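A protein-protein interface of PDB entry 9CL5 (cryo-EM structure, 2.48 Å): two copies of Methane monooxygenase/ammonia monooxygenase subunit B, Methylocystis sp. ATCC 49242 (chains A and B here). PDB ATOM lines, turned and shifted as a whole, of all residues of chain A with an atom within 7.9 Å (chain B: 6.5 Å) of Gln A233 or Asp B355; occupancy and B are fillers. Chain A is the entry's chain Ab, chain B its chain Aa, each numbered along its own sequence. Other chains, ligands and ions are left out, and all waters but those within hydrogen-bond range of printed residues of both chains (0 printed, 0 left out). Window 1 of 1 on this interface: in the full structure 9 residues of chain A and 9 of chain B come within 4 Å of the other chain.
O of Thr B356 is in hydrogen-bond range of N of Ala A234, at 3.4 Å.
The side-chain carboxylate (OD1) of Asp B357 lies within salt-bridge range of the guanidinium group (NH1) of Arg A80, at 2.9 Å.
N of Ser B358 sits at hydrogen-bond distance from OE1 of Gln A233.
The side-chain amide oxygen of Gln B7 lies close to the side-chain carboxylate of Asp B355 (2.9 Å).
The backbone NH (N) of Phe B9 sits at hydrogen-bond distance from the side-chain carboxylate (OD2) of Asp B355, at 3.2 Å.
OD2 of Asp B357 sits at hydrogen-bond distance from NE2 of Gln B359 (3.2 Å).
The guanidinium group (NH1) of Arg A80 sits at hydrogen-bond distance from the backbone carbonyl oxygen (O) of Ala A234.
O of Pro A231 lies within hydrogen-bond range of NE2 of Gln A233 (3.1 Å).
Among the printed residues, merely in contact across the chains: Leu A232 with Thr B356, Gln A233 with Thr B356, Pro A231 with Tyr B354, Pro A231 with Asp B355, Gln A233 with Asp B355, Pro A231 with Ala B353 and Gln A233 with Asp B357.
Of chain A, only Pro A231 and Gln A233 come within 4 Å of Asp B355.
Of the printed residues of chain B, Arg A80 touches Asp B357.
Printed residues of chain A within 4 Å of Ala B353: Pro A231.
Of the printed residues of chain A, Tyr B354 touches Pro A231.
Gly A235 touches none of the printed residues of chain B.
The nearest residue of chain B that does not touch Gln A233 is Ala B353 (6.1 Å).
The nearest residue of chain A that does not touch Asp B355 is Leu A232 (5.5 Å).
The nearest printed residue of chain B that does not touch Leu A232 is Asp B355 (5.5 Å).
Of the 14 printed residues of chain B, 6 touch a printed residue of chain A.
Printed residues of chain B that touch a printed residue of chain A: Ala B353, Tyr B354, Asp B355, Thr B356, Asp B357 and Ser B358.
Hydrophobic or aromatic side chains of chain A that line the printed part of chain B: Pro A231.
Among the printed residues, 10 pairs touch across the chains.
Among the printed residues, Asp or Glu carboxylates within 4 Å of a Lys or Arg side-chain nitrogen of the other chain: Arg A80 with Asp B357 (2.9 Å).
No position is printed for both chains.
Of the 10 pairs that touch across the chains among the printed residues, none has its exchanged pair printed and touching as well.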
ATOM      1  N   PRO A  79       5.818   9.722   0.109  1.00  0.00           N
ATOM      2  CA  PRO A  79       5.401  10.956  -0.567  1.00  0.00           C
ATOM      3  C   PRO A  79       4.196  11.623   0.074  1.00  0.00           C
ATOM      4  O   PRO A  79       3.889  12.771  -0.278  1.00  0.00           O
ATOM      5  CB  PRO A  79       5.074  10.484  -1.988  1.00  0.00           C
ATOM      6  CG  PRO A  79       4.827   9.019  -1.886  1.00  0.00           C
ATOM      7  CD  PRO A  79       5.273   8.520  -0.543  1.00  0.00           C
ATOM      8  N   ARG A  80       3.504  10.949   0.992  1.00  0.00           N
ATOM      9  CA  ARG A  80       2.359  11.540   1.671  1.00  0.00           C
ATOM     10  C   ARG A  80       2.522  11.466   3.183  1.00  0.00           C
ATOM     11  O   ARG A  80       3.593  11.113   3.684  1.00  0.00           O
ATOM     12  CB  ARG A  80       1.054  10.856   1.253  1.00  0.00           C
ATOM     13  CG  ARG A  80       1.094  10.140  -0.082  1.00  0.00           C
ATOM     14  CD  ARG A  80      -0.221   9.424  -0.324  1.00  0.00           C
ATOM     15  NE  ARG A  80      -0.140   8.437  -1.391  1.00  0.00           N
ATOM     16  CZ  ARG A  80      -1.041   7.487  -1.598  1.00  0.00           C
ATOM     17  NH1 ARG A  80      -2.103   7.362  -0.820  1.00  0.00           N
ATOM     18  NH2 ARG A  80      -0.872   6.640  -2.608  1.00  0.00           N
ATOM     19  N   ILE A 230      -5.146   9.376 -14.481  1.00  0.00           N
ATOM     20  CA  ILE A 230      -5.549   8.896 -13.162  1.00  0.00           C
ATOM     21  C   ILE A 230      -5.764  10.092 -12.243  1.00  0.00           C
ATOM     22  O   ILE A 230      -5.167  11.155 -12.467  1.00  0.00           O
ATOM     23  CB  ILE A 230      -4.509   7.923 -12.584  1.00  0.00           C
ATOM     24  CG1 ILE A 230      -3.134   8.588 -12.523  1.00  0.00           C
ATOM     25  CG2 ILE A 230      -4.449   6.647 -13.407  1.00  0.00           C
ATOM     26  CD1 ILE A 230      -2.210   7.975 -11.506  1.00  0.00           C
ATOM     27  N   PRO A 231      -6.603   9.979 -11.217  1.00  0.00           N
ATOM     28  CA  PRO A 231      -6.790  11.099 -10.288  1.00  0.00           C
ATOM     29  C   PRO A 231      -5.589  11.277  -9.372  1.00  0.00           C
ATOM     30  O   PRO A 231      -4.717  10.413  -9.262  1.00  0.00           O
ATOM     31  CB  PRO A 231      -8.040  10.719  -9.486  1.00  0.00           C
ATOM     32  CG  PRO A 231      -8.352   9.317  -9.818  1.00  0.00           C
ATOM     33  CD  PRO A 231      -7.490   8.838 -10.932  1.00  0.00           C
ATOM     34  N   LEU A 232      -5.557  12.432  -8.710  1.00  0.00           N
ATOM     35  CA  LEU A 232      -4.497  12.721  -7.754  1.00  0.00           C
ATOM     36  C   LEU A 232      -4.517  11.707  -6.617  1.00  0.00           C
ATOM     37  O   LEU A 232      -5.575  11.377  -6.076  1.00  0.00           O
ATOM     38  CB  LEU A 232      -4.657  14.135  -7.196  1.00  0.00           C
ATOM     39  CG  LEU A 232      -4.577  15.296  -8.187  1.00  0.00           C
ATOM     40  CD1 LEU A 232      -5.125  16.561  -7.555  1.00  0.00           C
ATOM     41  CD2 LEU A 232      -3.150  15.504  -8.652  1.00  0.00           C
ATOM     42  N   GLN A 233      -3.337  11.219  -6.250  1.00  0.00           N
ATOM     43  CA  GLN A 233      -3.193  10.180  -5.234  1.00  0.00           C
ATOM     44  C   GLN A 233      -2.936  10.845  -3.888  1.00  0.00           C
ATOM     45  O   GLN A 233      -1.946  11.566  -3.722  1.00  0.00           O
ATOM     46  CB  GLN A 233      -2.061   9.224  -5.604  1.00  0.00           C
ATOM     47  CG  GLN A 233      -2.174   8.656  -7.009  1.00  0.00           C
ATOM     48  CD  GLN A 233      -3.132   7.487  -7.093  1.00  0.00           C
ATOM     49  OE1 GLN A 233      -2.954   6.476  -6.417  1.00  0.00           O
ATOM     50  NE2 GLN A 233      -4.159   7.622  -7.923  1.00  0.00           N
ATOM     51  N   ALA A 234      -3.825  10.600  -2.926  1.00  0.00           N
ATOM     52  CA  ALA A 234      -3.736  11.223  -1.614  1.00  0.00           C
ATOM     53  C   ALA A 234      -4.209  10.245  -0.549  1.00  0.00           C
ATOM     54  O   ALA A 234      -4.949   9.299  -0.827  1.00  0.00           O
ATOM     55  CB  ALA A 234      -4.558  12.515  -1.549  1.00  0.00           C
ATOM     56  N   GLY A 235      -3.768  10.487   0.684  1.00  0.00           N
ATOM     57  CA  GLY A 235      -4.185   9.684   1.815  1.00  0.00           C
ATOM     58  C   GLY A 235      -3.061   9.349   2.776  1.00  0.00           C
ATOM     59  O   GLY A 235      -1.885   9.394   2.406  1.00  0.00           O
ATOM     60  N   GLN B   6     -19.443   0.858  -4.884  1.00  0.00           N
ATOM     61  CA  GLN B   6     -18.522   1.405  -3.869  1.00  0.00           C
ATOM     62  C   GLN B   6     -17.105   1.253  -4.413  1.00  0.00           C
ATOM     63  O   GLN B   6     -16.883   0.361  -5.231  1.00  0.00           O
ATOM     64  CB  GLN B   6     -18.756   0.697  -2.536  1.00  0.00           C
ATOM     65  CG  GLN B   6     -20.059   1.044  -1.829  1.00  0.00           C
ATOM     66  CD  GLN B   6     -20.169   0.385  -0.473  1.00  0.00           C
ATOM     67  OE1 GLN B   6     -20.115  -0.842  -0.347  1.00  0.00           O
ATOM     68  NE2 GLN B   6     -20.309   1.192   0.565  1.00  0.00           N
ATOM     69  N   GLN B   7     -16.190   2.114  -3.981  1.00  0.00           N
ATOM     70  CA  GLN B   7     -14.827   2.071  -4.493  1.00  0.00           C
ATOM     71  C   GLN B   7     -14.151   0.762  -4.110  1.00  0.00           C
ATOM     72  O   GLN B   7     -14.338   0.246  -3.005  1.00  0.00           O
ATOM     73  CB  GLN B   7     -14.024   3.256  -3.961  1.00  0.00           C
ATOM     74  CG  GLN B   7     -14.835   4.526  -3.801  1.00  0.00           C
ATOM     75  CD  GLN B   7     -14.052   5.768  -4.165  1.00  0.00           C
ATOM     76  OE1 GLN B   7     -13.154   5.727  -5.003  1.00  0.00           O
ATOM     77  NE2 GLN B   7     -14.390   6.883  -3.533  1.00  0.00           N
ATOM     78  N   ALA B   8     -13.365   0.223  -5.043  1.00  0.00           N
ATOM     79  CA  ALA B   8     -12.736  -1.076  -4.828  1.00  0.00           C
ATOM     80  C   ALA B   8     -11.737  -1.033  -3.680  1.00  0.00           C
ATOM     81  O   ALA B   8     -11.684  -1.955  -2.859  1.00  0.00           O
ATOM     82  CB  ALA B   8     -12.053  -1.543  -6.113  1.00  0.00           C
ATOM     83  N   PHE B   9     -10.934   0.031  -3.605  1.00  0.00           N
ATOM     84  CA  PHE B   9      -9.874   0.077  -2.603  1.00  0.00           C
ATOM     85  C   PHE B   9     -10.432   0.257  -1.197  1.00  0.00           C
ATOM     86  O   PHE B   9      -9.810  -0.189  -0.228  1.00  0.00           O
ATOM     87  CB  PHE B   9      -8.868   1.179  -2.951  1.00  0.00           C
ATOM     88  CG  PHE B   9      -9.136   2.501  -2.284  1.00  0.00           C
ATOM     89  CD1 PHE B   9      -9.999   3.418  -2.859  1.00  0.00           C
ATOM     90  CD2 PHE B   9      -8.497   2.839  -1.103  1.00  0.00           C
ATOM     91  CE1 PHE B   9     -10.238   4.637  -2.257  1.00  0.00           C
ATOM     92  CE2 PHE B   9      -8.735   4.054  -0.495  1.00  0.00           C
ATOM     93  CZ  PHE B   9      -9.606   4.955  -1.075  1.00  0.00           C
ATOM     94  N   LEU B  10     -11.591   0.899  -1.063  1.00  0.00           N
ATOM     95  CA  LEU B  10     -12.221   1.004   0.248  1.00  0.00           C
ATOM     96  C   LEU B  10     -12.888  -0.305   0.648  1.00  0.00           C
ATOM     97  O   LEU B  10     -12.891  -0.667   1.829  1.00  0.00           O
ATOM     98  CB  LEU B  10     -13.234   2.146   0.251  1.00  0.00           C
ATOM     99  CG  LEU B  10     -12.628   3.547   0.236  1.00  0.00           C
ATOM    100  CD1 LEU B  10     -13.701   4.586   0.015  1.00  0.00           C
ATOM    101  CD2 LEU B  10     -11.880   3.818   1.526  1.00  0.00           C
ATOM    102  N   ASP B 351     -12.126  -1.401 -11.305  1.00  0.00           N
ATOM    103  CA  ASP B 351     -12.226   0.051 -11.270  1.00  0.00           C
ATOM    104  C   ASP B 351     -11.229   0.682 -10.307  1.00  0.00           C
ATOM    105  O   ASP B 351     -11.383   1.856  -9.956  1.00  0.00           O
ATOM    106  CB  ASP B 351     -13.649   0.473 -10.896  1.00  0.00           C
ATOM    107  CG  ASP B 351     -14.633   0.264 -12.028  1.00  0.00           C
ATOM    108  OD1 ASP B 351     -14.458  -0.700 -12.801  1.00  0.00           O
ATOM    109  OD2 ASP B 351     -15.581   1.068 -12.145  1.00  0.00           O
ATOM    110  N   LEU B 352     -10.221  -0.082  -9.876  1.00  0.00           N
ATOM    111  CA  LEU B 352      -9.174   0.452  -9.011  1.00  0.00           C
ATOM    112  C   LEU B 352      -8.486   1.658  -9.639  1.00  0.00           C
ATOM    113  O   LEU B 352      -8.013   2.545  -8.921  1.00  0.00           O
ATOM    114  CB  LEU B 352      -8.154  -0.644  -8.707  1.00  0.00           C
ATOM    115  CG  LEU B 352      -7.228  -0.487  -7.504  1.00  0.00           C
ATOM    116  CD1 LEU B 352      -7.966   0.105  -6.317  1.00  0.00           C
ATOM    117  CD2 LEU B 352      -6.626  -1.833  -7.146  1.00  0.00           C
ATOM    118  N   ALA B 353      -8.423   1.709 -10.970  1.00  0.00           N
ATOM    119  CA  ALA B 353      -7.791   2.826 -11.657  1.00  0.00           C
ATOM    120  C   ALA B 353      -8.583   4.120 -11.540  1.00  0.00           C
ATOM    121  O   ALA B 353      -8.056   5.180 -11.893  1.00  0.00           O
ATOM    122  CB  ALA B 353      -7.578   2.480 -13.131  1.00  0.00           C
ATOM    123  N   TYR B 354      -9.828   4.065 -11.068  1.00  0.00           N
ATOM    124  CA  TYR B 354     -10.610   5.270 -10.834  1.00  0.00           C
ATOM    125  C   TYR B 354     -10.409   5.843  -9.438  1.00  0.00           C
ATOM    126  O   TYR B 354     -10.779   6.996  -9.197  1.00  0.00           O
ATOM    127  CB  TYR B 354     -12.100   4.984 -11.062  1.00  0.00           C
ATOM    128  CG  TYR B 354     -12.973   6.217 -11.028  1.00  0.00           C
ATOM    129  CD1 TYR B 354     -12.990   7.110 -12.091  1.00  0.00           C
ATOM    130  CD2 TYR B 354     -13.776   6.494  -9.928  1.00  0.00           C
ATOM    131  CE1 TYR B 354     -13.785   8.238 -12.063  1.00  0.00           C
ATOM    132  CE2 TYR B 354     -14.572   7.621  -9.889  1.00  0.00           C
ATOM    133  CZ  TYR B 354     -14.571   8.490 -10.959  1.00  0.00           C
ATOM    134  OH  TYR B 354     -15.363   9.614 -10.926  1.00  0.00           O
ATOM    135  N   ASP B 355      -9.816   5.080  -8.525  1.00  0.00           N
ATOM    136  CA  ASP B 355      -9.686   5.503  -7.142  1.00  0.00           C
ATOM    137  C   ASP B 355      -8.490   6.433  -6.963  1.00  0.00           C
ATOM    138  O   ASP B 355      -7.594   6.514  -7.806  1.00  0.00           O
ATOM    139  CB  ASP B 355      -9.539   4.291  -6.223  1.00  0.00           C
ATOM    140  CG  ASP B 355     -10.721   3.346  -6.307  1.00  0.00           C
ATOM    141  OD1 ASP B 355     -11.805   3.780  -6.751  1.00  0.00           O
ATOM    142  OD2 ASP B 355     -10.566   2.167  -5.929  1.00  0.00           O
ATOM    143  N   THR B 356      -8.489   7.141  -5.834  1.00  0.00           N
ATOM    144  CA  THR B 356      -7.380   8.003  -5.457  1.00  0.00           C
ATOM    145  C   THR B 356      -6.299   7.264  -4.681  1.00  0.00           C
ATOM    146  O   THR B 356      -5.328   7.891  -4.249  1.00  0.00           O
ATOM    147  CB  THR B 356      -7.886   9.186  -4.629  1.00  0.00           C
ATOM    148  OG1 THR B 356      -8.893   8.736  -3.715  1.00  0.00           O
ATOM    149  CG2 THR B 356      -8.477  10.249  -5.536  1.00  0.00           C
ATOM    150  N   ASP B 357      -6.453   5.955  -4.483  1.00  0.00           N
ATOM    151  CA  ASP B 357      -5.437   5.125  -3.836  1.00  0.00           C
ATOM    152  C   ASP B 357      -5.461   3.767  -4.529  1.00  0.00           C
ATOM    153  O   ASP B 357      -6.361   2.957  -4.286  1.00  0.00           O
ATOM    154  CB  ASP B 357      -5.697   4.996  -2.341  1.00  0.00           C
ATOM    155  CG  ASP B 357      -4.421   4.973  -1.528  1.00  0.00           C
ATOM    156  OD1 ASP B 357      -3.329   5.025  -2.132  1.00  0.00           O
ATOM    157  OD2 ASP B 357      -4.508   4.904  -0.284  1.00  0.00           O
ATOM    158  N   SER B 358      -4.475   3.523  -5.392  1.00  0.00           N
ATOM    159  CA  SER B 358      -4.401   2.281  -6.162  1.00  0.00           C
ATOM    160  C   SER B 358      -3.726   1.201  -5.316  1.00  0.00           C
ATOM    161  O   SER B 358      -2.555   0.856  -5.486  1.00  0.00           O
ATOM    162  CB  SER B 358      -3.664   2.510  -7.474  1.00  0.00           C
ATOM    163  OG  SER B 358      -4.058   1.569  -8.456  1.00  0.00           O
ATOM    164  N   GLN B 359      -4.502   0.659  -4.381  1.00  0.00           N
ATOM    165  CA  GLN B 359      -4.028  -0.358  -3.457  1.00  0.00           C
ATOM    166  C   GLN B 359      -5.006  -1.524  -3.414  1.00  0.00           C
ATOM    167  O   GLN B 359      -6.206  -1.361  -3.651  1.00  0.00           O
ATOM    168  CB  GLN B 359      -3.853   0.209  -2.042  1.00  0.00           C
ATOM    169  CG  GLN B 359      -3.135   1.540  -1.978  1.00  0.00           C
ATOM    170  CD  GLN B 359      -2.171   1.621  -0.819  1.00  0.00           C
ATOM    171  OE1 GLN B 359      -1.305   0.765  -0.656  1.00  0.00           O
ATOM    172  NE2 GLN B 359      -2.316   2.654  -0.003  1.00  0.00           N
